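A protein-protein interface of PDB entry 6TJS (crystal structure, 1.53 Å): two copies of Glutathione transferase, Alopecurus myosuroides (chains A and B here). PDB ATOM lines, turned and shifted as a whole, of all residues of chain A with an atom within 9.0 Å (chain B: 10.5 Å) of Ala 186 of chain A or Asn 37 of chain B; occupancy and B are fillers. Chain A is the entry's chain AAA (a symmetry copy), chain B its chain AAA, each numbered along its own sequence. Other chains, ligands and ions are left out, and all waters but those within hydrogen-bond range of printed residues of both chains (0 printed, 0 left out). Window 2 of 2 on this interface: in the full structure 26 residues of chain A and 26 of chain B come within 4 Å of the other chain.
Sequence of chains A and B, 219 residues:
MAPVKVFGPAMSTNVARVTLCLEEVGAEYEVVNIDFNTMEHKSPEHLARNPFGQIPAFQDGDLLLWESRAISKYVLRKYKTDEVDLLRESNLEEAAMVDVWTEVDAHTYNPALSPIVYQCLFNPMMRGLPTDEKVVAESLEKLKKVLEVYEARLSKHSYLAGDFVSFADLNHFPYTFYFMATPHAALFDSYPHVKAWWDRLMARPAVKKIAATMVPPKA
Ala 181 of chain A touches Pro 217 of chain B (CB to CD, 3.7 Å).
Pro 183 of chain A touches Ile 34 of chain B.
CE1 of His 184 of chain A touches CD2 of Phe 36 of chain B (3.0 Å).
Asn 37 of chain B touches Ala 186 of chain A (OD1 to CB, 3.4 Å).
The side-chain hydroxyl of Thr 182 of chain A lies close to the backbone NH of His 184 of chain A (3.1 Å).
No position is printed for both chains.
Of the 8 pairs that touch across the chains among the printed residues, none has its exchanged pair printed and touching as well.
Leu 147 of chain A touches none of the printed residues of chain B.
Ala 186 of chain A touches two residues of chain B.
No residue of chain B comes within 4 Å of Leu 187 of chain A.
No residue of chain B comes within 4 Å of Asp 189 of chain A.
Pro 192 of chain A touches none of the printed residues of chain B.
Of the printed residues of chain A, Ile 34 of chain B touches Pro 183.
Of the printed residues of chain A, Asp 35 of chain B touches Pro 183, Ala 185 and Ala 186.
Of chain A, only Ala 186 (3.4 Å) comes within 4 Å of Asn 37 of chain B.
The nearest residue of chain B that does not touch Ala 186 of chain A is Phe 36 of chain B (5.8 Å).
The nearest residue of chain A that does not touch Asn 37 of chain B is Leu 187 of chain A (4.9 Å).
The nearest printed residue of chain B that does not touch Pro 183 of chain A is Ile 55 of chain B (4.2 Å).
Printed residues of chain A that touch a printed residue of chain B: Ala 181, Pro 183, His 184, Ala 185 and Ala 186.
Hydrophobic or aromatic side chains of chain A that line the printed part of chain B: Ala 181, Pro 183, His 184, Ala 185 and Ala 186.
Among the printed residues, 8 pairs touch across the chains.
Among the printed residues, no Asp or Glu carboxylate lies within 4 Å of a Lys or Arg side-chain nitrogen of the other chain.
The side-chain carboxylate (OD1) of Asp 35 of chain B sits at hydrogen-bond distance from the backbone NH (N) of Ala 185 of chain A, 3.3 Å away.
The side-chain carboxylate (OD1) of Asp 35 of chain B is in hydrogen-bond range of the backbone NH (N) of Ala 186 of chain A (3.0 Å).
The backbone NH (N) of Phe 36 of chain B is in hydrogen-bond range of the backbone carbonyl oxygen (O) of Pro 183 of chain A (2.8 Å).
The backbone carbonyl oxygen (O) of Pro 183 of chain A sits close to the side-chain carboxylate (OD1) of Asp 35 of chain B (3.2 Å).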
ATOM      1  N   LEU A 140       2.081  17.399   0.631  1.00  0.00           N
ATOM      2  CA  LEU A 140       3.093  18.255  -0.032  1.00  0.00           C
ATOM      3  C   LEU A 140       4.311  18.417   0.880  1.00  0.00           C
ATOM      4  O   LEU A 140       5.422  18.449   0.363  1.00  0.00           O
ATOM      5  CB  LEU A 140       2.509  19.633  -0.364  1.00  0.00           C
ATOM      6  CG  LEU A 140       1.708  19.769  -1.661  1.00  0.00           C
ATOM      7  CD1 LEU A 140       2.321  18.955  -2.800  1.00  0.00           C
ATOM      8  CD2 LEU A 140       0.255  19.378  -1.453  1.00  0.00           C
ATOM      9  N   LEU A 147      11.857  15.130  -1.546  1.00  0.00           N
ATOM     10  CA  LEU A 147      12.539  15.758  -2.696  1.00  0.00           C
ATOM     11  C   LEU A 147      13.868  16.421  -2.278  1.00  0.00           C
ATOM     12  O   LEU A 147      14.783  16.472  -3.072  1.00  0.00           O
ATOM     13  CB  LEU A 147      11.615  16.737  -3.410  1.00  0.00           C
ATOM     14  CG  LEU A 147      10.438  16.073  -4.142  1.00  0.00           C
ATOM     15  CD1 LEU A 147       9.536  17.089  -4.739  1.00  0.00           C
ATOM     16  CD2 LEU A 147      10.961  15.077  -5.198  1.00  0.00           C
ATOM     17  N   PHE A 179       1.796  12.156 -11.335  1.00  0.00           N
ATOM     18  CA  PHE A 179       2.029  13.412 -10.563  1.00  0.00           C
ATOM     19  C   PHE A 179       2.204  14.590 -11.481  1.00  0.00           C
ATOM     20  O   PHE A 179       1.658  15.696 -11.187  1.00  0.00           O
ATOM     21  CB  PHE A 179       3.196  13.228  -9.605  1.00  0.00           C
ATOM     22  CG  PHE A 179       3.505  14.501  -8.859  1.00  0.00           C
ATOM     23  CD1 PHE A 179       2.858  14.774  -7.688  1.00  0.00           C
ATOM     24  CD2 PHE A 179       4.420  15.397  -9.361  1.00  0.00           C
ATOM     25  CE1 PHE A 179       3.192  15.912  -6.957  1.00  0.00           C
ATOM     26  CE2 PHE A 179       4.725  16.550  -8.649  1.00  0.00           C
ATOM     27  CZ  PHE A 179       4.104  16.796  -7.470  1.00  0.00           C
ATOM     28  N   MET A 180       2.895  14.399 -12.600  1.00  0.00           N
ATOM     29  CA  MET A 180       3.178  15.465 -13.577  1.00  0.00           C
ATOM     30  C   MET A 180       1.911  15.893 -14.357  1.00  0.00           C
ATOM     31  O   MET A 180       1.914  16.956 -15.020  1.00  0.00           O
ATOM     32  CB  MET A 180       4.314  15.043 -14.507  1.00  0.00           C
ATOM     33  CG  MET A 180       5.590  14.868 -13.760  1.00  0.00           C
ATOM     34  SD  MET A 180       6.104  16.508 -13.087  1.00  0.00           S
ATOM     35  CE  MET A 180       7.503  16.043 -12.078  1.00  0.00           C
ATOM     36  N   ALA A 181       0.806  15.155 -14.212  1.00  0.00           N
ATOM     37  CA  ALA A 181      -0.500  15.534 -14.797  1.00  0.00           C
ATOM     38  C   ALA A 181      -1.291  16.434 -13.837  1.00  0.00           C
ATOM     39  O   ALA A 181      -2.337  16.991 -14.256  1.00  0.00           O
ATOM     40  CB  ALA A 181      -1.297  14.328 -15.139  1.00  0.00           C
ATOM     41  N   THR A 182      -0.837  16.576 -12.607  1.00  0.00           N
ATOM     42  CA  THR A 182      -1.541  17.377 -11.574  1.00  0.00           C
ATOM     43  C   THR A 182      -1.030  18.803 -11.605  1.00  0.00           C
ATOM     44  O   THR A 182       0.028  19.088 -12.133  1.00  0.00           O
ATOM     45  CB  THR A 182      -1.326  16.834 -10.184  1.00  0.00           C
ATOM     46  OG1 THR A 182      -0.021  17.104  -9.672  1.00  0.00           O
ATOM     47  CG2 THR A 182      -1.689  15.372 -10.138  1.00  0.00           C
ATOM     48  N   PRO A 183      -1.757  19.721 -10.957  1.00  0.00           N
ATOM     49  CA  PRO A 183      -1.276  21.089 -10.851  1.00  0.00           C
ATOM     50  C   PRO A 183      -0.116  21.249  -9.874  1.00  0.00           C
ATOM     51  O   PRO A 183       0.271  22.360  -9.621  1.00  0.00           O
ATOM     52  CB  PRO A 183      -2.478  21.837 -10.299  1.00  0.00           C
ATOM     53  CG  PRO A 183      -3.664  20.968 -10.575  1.00  0.00           C
ATOM     54  CD  PRO A 183      -3.138  19.549 -10.473  1.00  0.00           C
ATOM     55  N   HIS A 184       0.341  20.181  -9.237  1.00  0.00           N
ATOM     56  CA  HIS A 184       1.574  20.212  -8.405  1.00  0.00           C
ATOM     57  C   HIS A 184       2.817  19.880  -9.223  1.00  0.00           C
ATOM     58  O   HIS A 184       3.909  19.887  -8.592  1.00  0.00           O
ATOM     59  CB  HIS A 184       1.477  19.281  -7.213  1.00  0.00           C
ATOM     60  CG  HIS A 184       0.491  19.771  -6.217  1.00  0.00           C
ATOM     61  ND1 HIS A 184       0.734  20.892  -5.439  1.00  0.00           N
ATOM     62  CD2 HIS A 184      -0.740  19.335  -5.912  1.00  0.00           C
ATOM     63  CE1 HIS A 184      -0.316  21.108  -4.681  1.00  0.00           C
ATOM     64  NE2 HIS A 184      -1.226  20.166  -4.956  1.00  0.00           N
ATOM     65  N   ALA A 185       2.717  19.681 -10.536  1.00  0.00           N
ATOM     66  CA  ALA A 185       3.872  19.256 -11.375  1.00  0.00           C
ATOM     67  C   ALA A 185       5.049  20.219 -11.148  1.00  0.00           C
ATOM     68  O   ALA A 185       6.174  19.760 -10.968  1.00  0.00           O
ATOM     69  CB  ALA A 185       3.519  19.190 -12.826  1.00  0.00           C
ATOM     70  N   ALA A 186       4.790  21.518 -11.084  1.00  0.00           N
ATOM     71  CA  ALA A 186       5.874  22.540 -11.012  1.00  0.00           C
ATOM     72  C   ALA A 186       6.661  22.413  -9.703  1.00  0.00           C
ATOM     73  O   ALA A 186       7.710  23.072  -9.605  1.00  0.00           O
ATOM     74  CB  ALA A 186       5.280  23.940 -11.100  1.00  0.00           C
ATOM     75  N   LEU A 187       6.206  21.652  -8.714  1.00  0.00           N
ATOM     76  CA  LEU A 187       6.961  21.482  -7.434  1.00  0.00           C
ATOM     77  C   LEU A 187       8.398  21.056  -7.737  1.00  0.00           C
ATOM     78  O   LEU A 187       9.368  21.452  -7.023  1.00  0.00           O
ATOM     79  CB  LEU A 187       6.300  20.422  -6.567  1.00  0.00           C
ATOM     80  CG  LEU A 187       6.988  20.156  -5.232  1.00  0.00           C
ATOM     81  CD1 LEU A 187       7.086  21.431  -4.380  1.00  0.00           C
ATOM     82  CD2 LEU A 187       6.224  19.062  -4.504  1.00  0.00           C
ATOM     83  N   PHE A 188       8.577  20.209  -8.748  1.00  0.00           N
ATOM     84  CA  PHE A 188       9.925  19.694  -9.083  1.00  0.00           C
ATOM     85  C   PHE A 188      10.864  20.824  -9.505  1.00  0.00           C
ATOM     86  O   PHE A 188      12.097  20.672  -9.409  1.00  0.00           O
ATOM     87  CB  PHE A 188       9.871  18.607 -10.165  1.00  0.00           C
ATOM     88  CG  PHE A 188       9.589  17.229  -9.650  1.00  0.00           C
ATOM     89  CD1 PHE A 188       8.689  16.962  -8.654  1.00  0.00           C
ATOM     90  CD2 PHE A 188      10.186  16.157 -10.298  1.00  0.00           C
ATOM     91  CE1 PHE A 188       8.406  15.659  -8.256  1.00  0.00           C
ATOM     92  CE2 PHE A 188       9.880  14.862  -9.923  1.00  0.00           C
ATOM     93  CZ  PHE A 188       9.059  14.611  -8.868  1.00  0.00           C
ATOM     94  N   ASP A 189      10.326  21.977  -9.916  1.00  0.00           N
ATOM     95  CA  ASP A 189      11.178  23.108 -10.342  1.00  0.00           C
ATOM     96  C   ASP A 189      11.980  23.629  -9.127  1.00  0.00           C
ATOM     97  O   ASP A 189      13.025  24.264  -9.404  1.00  0.00           O
ATOM     98  CB  ASP A 189      10.369  24.232 -10.980  1.00  0.00           C
ATOM     99  CG  ASP A 189       9.676  23.821 -12.259  1.00  0.00           C
ATOM    100  OD1 ASP A 189       9.956  22.719 -12.772  1.00  0.00           O
ATOM    101  OD2 ASP A 189       8.834  24.598 -12.696  1.00  0.00           O
ATOM    102  N   SER A 190      11.545  23.413  -7.898  1.00  0.00           N
ATOM    103  CA  SER A 190      12.236  23.824  -6.654  1.00  0.00           C
ATOM    104  C   SER A 190      13.408  22.880  -6.350  1.00  0.00           C
ATOM    105  O   SER A 190      14.106  23.118  -5.382  1.00  0.00           O
ATOM    106  CB  SER A 190      11.261  23.874  -5.496  1.00  0.00           C
ATOM    107  OG  SER A 190      10.305  24.892  -5.733  1.00  0.00           O
ATOM    108  N   TYR A 191      13.561  21.787  -7.123  1.00  0.00           N
ATOM    109  CA  TYR A 191      14.598  20.765  -6.905  1.00  0.00           C
ATOM    110  C   TYR A 191      15.276  20.512  -8.240  1.00  0.00           C
ATOM    111  O   TYR A 191      14.978  19.537  -8.930  1.00  0.00           O
ATOM    112  CB  TYR A 191      14.001  19.522  -6.256  1.00  0.00           C
ATOM    113  CG  TYR A 191      13.203  19.852  -5.016  1.00  0.00           C
ATOM    114  CD1 TYR A 191      13.827  19.964  -3.780  1.00  0.00           C
ATOM    115  CD2 TYR A 191      11.842  20.129  -5.117  1.00  0.00           C
ATOM    116  CE1 TYR A 191      13.095  20.327  -2.660  1.00  0.00           C
ATOM    117  CE2 TYR A 191      11.104  20.434  -3.990  1.00  0.00           C
ATOM    118  CZ  TYR A 191      11.741  20.576  -2.774  1.00  0.00           C
ATOM    119  OH  TYR A 191      11.018  20.918  -1.660  1.00  0.00           O
ATOM    120  N   PRO A 192      16.178  21.413  -8.666  1.00  0.00           N
ATOM    121  CA  PRO A 192      16.622  21.419 -10.043  1.00  0.00           C
ATOM    122  C   PRO A 192      17.306  20.132 -10.513  1.00  0.00           C
ATOM    123  O   PRO A 192      17.184  19.796 -11.660  1.00  0.00           O
ATOM    124  CB  PRO A 192      17.666  22.534 -10.093  1.00  0.00           C
ATOM    125  CG  PRO A 192      17.313  23.432  -8.963  1.00  0.00           C
ATOM    126  CD  PRO A 192      16.644  22.592  -7.894  1.00  0.00           C
ATOM    127  N   LYS A 195      14.393  17.714 -11.087  1.00  0.00           N
ATOM    128  CA  LYS A 195      13.776  18.103 -12.361  1.00  0.00           C
ATOM    129  C   LYS A 195      14.630  17.599 -13.531  1.00  0.00           C
ATOM    130  O   LYS A 195      14.081  17.018 -14.476  1.00  0.00           O
ATOM    131  CB  LYS A 195      13.586  19.617 -12.445  1.00  0.00           C
ATOM    132  CG  LYS A 195      12.990  20.103 -13.779  1.00  0.00           C
ATOM    133  CD  LYS A 195      13.048  21.641 -13.832  1.00  0.00           C
ATOM    134  CE  LYS A 195      12.450  22.336 -15.048  1.00  0.00           C
ATOM    135  NZ  LYS A 195      11.031  22.003 -15.230  1.00  0.00           N
ATOM    136  N   PHE B   7      -9.896  25.864 -15.868  1.00  0.00           N
ATOM    137  CA  PHE B   7      -8.527  25.693 -15.380  1.00  0.00           C
ATOM    138  C   PHE B   7      -8.380  24.389 -14.599  1.00  0.00           C
ATOM    139  O   PHE B   7      -9.091  24.194 -13.604  1.00  0.00           O
ATOM    140  CB  PHE B   7      -8.114  26.884 -14.529  1.00  0.00           C
ATOM    141  CG  PHE B   7      -8.203  28.237 -15.186  1.00  0.00           C
ATOM    142  CD1 PHE B   7      -9.343  28.993 -15.093  1.00  0.00           C
ATOM    143  CD2 PHE B   7      -7.083  28.781 -15.801  1.00  0.00           C
ATOM    144  CE1 PHE B   7      -9.421  30.245 -15.699  1.00  0.00           C
ATOM    145  CE2 PHE B   7      -7.157  30.041 -16.399  1.00  0.00           C
ATOM    146  CZ  PHE B   7      -8.314  30.765 -16.344  1.00  0.00           C
ATOM    147  N   ASN B  33      -4.116  24.364 -18.551  1.00  0.00           N
ATOM    148  CA  ASN B  33      -3.399  23.516 -17.580  1.00  0.00           C
ATOM    149  C   ASN B  33      -2.675  24.499 -16.683  1.00  0.00           C
ATOM    150  O   ASN B  33      -1.799  25.197 -17.207  1.00  0.00           O
ATOM    151  CB  ASN B  33      -2.447  22.537 -18.280  1.00  0.00           C
ATOM    152  CG  ASN B  33      -2.149  21.280 -17.484  1.00  0.00           C
ATOM    153  OD1 ASN B  33      -2.818  20.956 -16.499  1.00  0.00           O
ATOM    154  ND2 ASN B  33      -1.119  20.559 -17.909  1.00  0.00           N
ATOM    155  N   ILE B  34      -3.078  24.640 -15.428  1.00  0.00           N
ATOM    156  CA  ILE B  34      -2.369  25.544 -14.479  1.00  0.00           C
ATOM    157  C   ILE B  34      -1.612  24.713 -13.441  1.00  0.00           C
ATOM    158  O   ILE B  34      -2.033  23.598 -13.088  1.00  0.00           O
ATOM    159  CB  ILE B  34      -3.338  26.547 -13.824  1.00  0.00           C
ATOM    160  CG1 ILE B  34      -4.509  25.853 -13.133  1.00  0.00           C
ATOM    161  CG2 ILE B  34      -3.809  27.574 -14.838  1.00  0.00           C
ATOM    162  CD1 ILE B  34      -5.072  26.638 -11.969  1.00  0.00           C
ATOM    163  N   ASP B  35      -0.522  25.291 -12.949  1.00  0.00           N
ATOM    164  CA  ASP B  35       0.295  24.786 -11.834  1.00  0.00           C
ATOM    165  C   ASP B  35      -0.047  25.666 -10.643  1.00  0.00           C
ATOM    166  O   ASP B  35      -0.233  26.871 -10.872  1.00  0.00           O
ATOM    167  CB  ASP B  35       1.776  24.868 -12.213  1.00  0.00           C
ATOM    168  CG  ASP B  35       2.302  23.598 -12.856  1.00  0.00           C
ATOM    169  OD1 ASP B  35       2.240  22.536 -12.179  1.00  0.00           O
ATOM    170  OD2 ASP B  35       2.772  23.677 -14.022  1.00  0.00           O
ATOM    171  N   PHE B  36      -0.117  25.113  -9.441  1.00  0.00           N
ATOM    172  CA  PHE B  36      -0.442  25.878  -8.209  1.00  0.00           C
ATOM    173  C   PHE B  36       0.615  26.964  -7.892  1.00  0.00           C
ATOM    174  O   PHE B  36       0.743  27.294  -6.706  1.00  0.00           O
ATOM    175  CB  PHE B  36      -0.587  24.928  -7.017  1.00  0.00           C
ATOM    176  CG  PHE B  36      -1.839  24.099  -6.996  1.00  0.00           C
ATOM    177  CD1 PHE B  36      -3.083  24.689  -7.122  1.00  0.00           C
ATOM    178  CD2 PHE B  36      -1.783  22.734  -6.774  1.00  0.00           C
ATOM    179  CE1 PHE B  36      -4.233  23.920  -7.090  1.00  0.00           C
ATOM    180  CE2 PHE B  36      -2.938  21.970  -6.726  1.00  0.00           C
ATOM    181  CZ  PHE B  36      -4.164  22.568  -6.887  1.00  0.00           C
ATOM    182  N   ASN B  37       1.313  27.568  -8.867  1.00  0.00           N
ATOM    183  CA  ASN B  37       2.251  28.704  -8.598  1.00  0.00           C
ATOM    184  C   ASN B  37       2.370  29.624  -9.820  1.00  0.00           C
ATOM    185  O   ASN B  37       1.330  30.185 -10.206  1.00  0.00           O
ATOM    186  CB  ASN B  37       3.634  28.210  -8.173  1.00  0.00           C
ATOM    187  CG  ASN B  37       4.264  27.275  -9.182  1.00  0.00           C
ATOM    188  OD1 ASN B  37       5.106  26.465  -8.817  1.00  0.00           O
ATOM    189  ND2 ASN B  37       3.879  27.378 -10.446  1.00  0.00           N
ATOM    190  N   GLY B  53      -7.973  28.496  -3.316  1.00  0.00           N
ATOM    191  CA  GLY B  53      -6.985  28.096  -4.340  1.00  0.00           C
ATOM    192  C   GLY B  53      -7.336  26.750  -4.951  1.00  0.00           C
ATOM    193  O   GLY B  53      -6.444  25.885  -5.058  1.00  0.00           O
ATOM    194  N   ILE B  55      -8.990  23.907  -7.814  1.00  0.00           N
ATOM    195  CA  ILE B  55      -9.008  23.486  -9.235  1.00  0.00           C
ATOM    196  C   ILE B  55     -10.049  22.376  -9.277  1.00  0.00           C
ATOM    197  O   ILE B  55     -10.089  21.582  -8.341  1.00  0.00           O
ATOM    198  CB  ILE B  55      -7.591  23.033  -9.698  1.00  0.00           C
ATOM    199  CG1 ILE B  55      -6.660  24.191 -10.076  1.00  0.00           C
ATOM    200  CG2 ILE B  55      -7.692  22.066 -10.853  1.00  0.00           C
ATOM    201  CD1 ILE B  55      -6.384  25.181  -8.987  1.00  0.00           C
ATOM    202  N   PRO B 217      -1.016  14.936 -19.999  1.00  0.00           N
ATOM    203  CA  PRO B 217      -0.528  15.911 -20.985  1.00  0.00           C
ATOM    204  C   PRO B 217       0.674  15.348 -21.772  1.00  0.00           C
ATOM    205  O   PRO B 217       1.344  14.472 -21.305  1.00  0.00           O
ATOM    206  CB  PRO B 217      -0.236  17.162 -20.139  1.00  0.00           C
ATOM    207  CG  PRO B 217       0.069  16.638 -18.754  1.00  0.00           C
ATOM    208  CD  PRO B 217      -0.758  15.367 -18.619  1.00  0.00           C
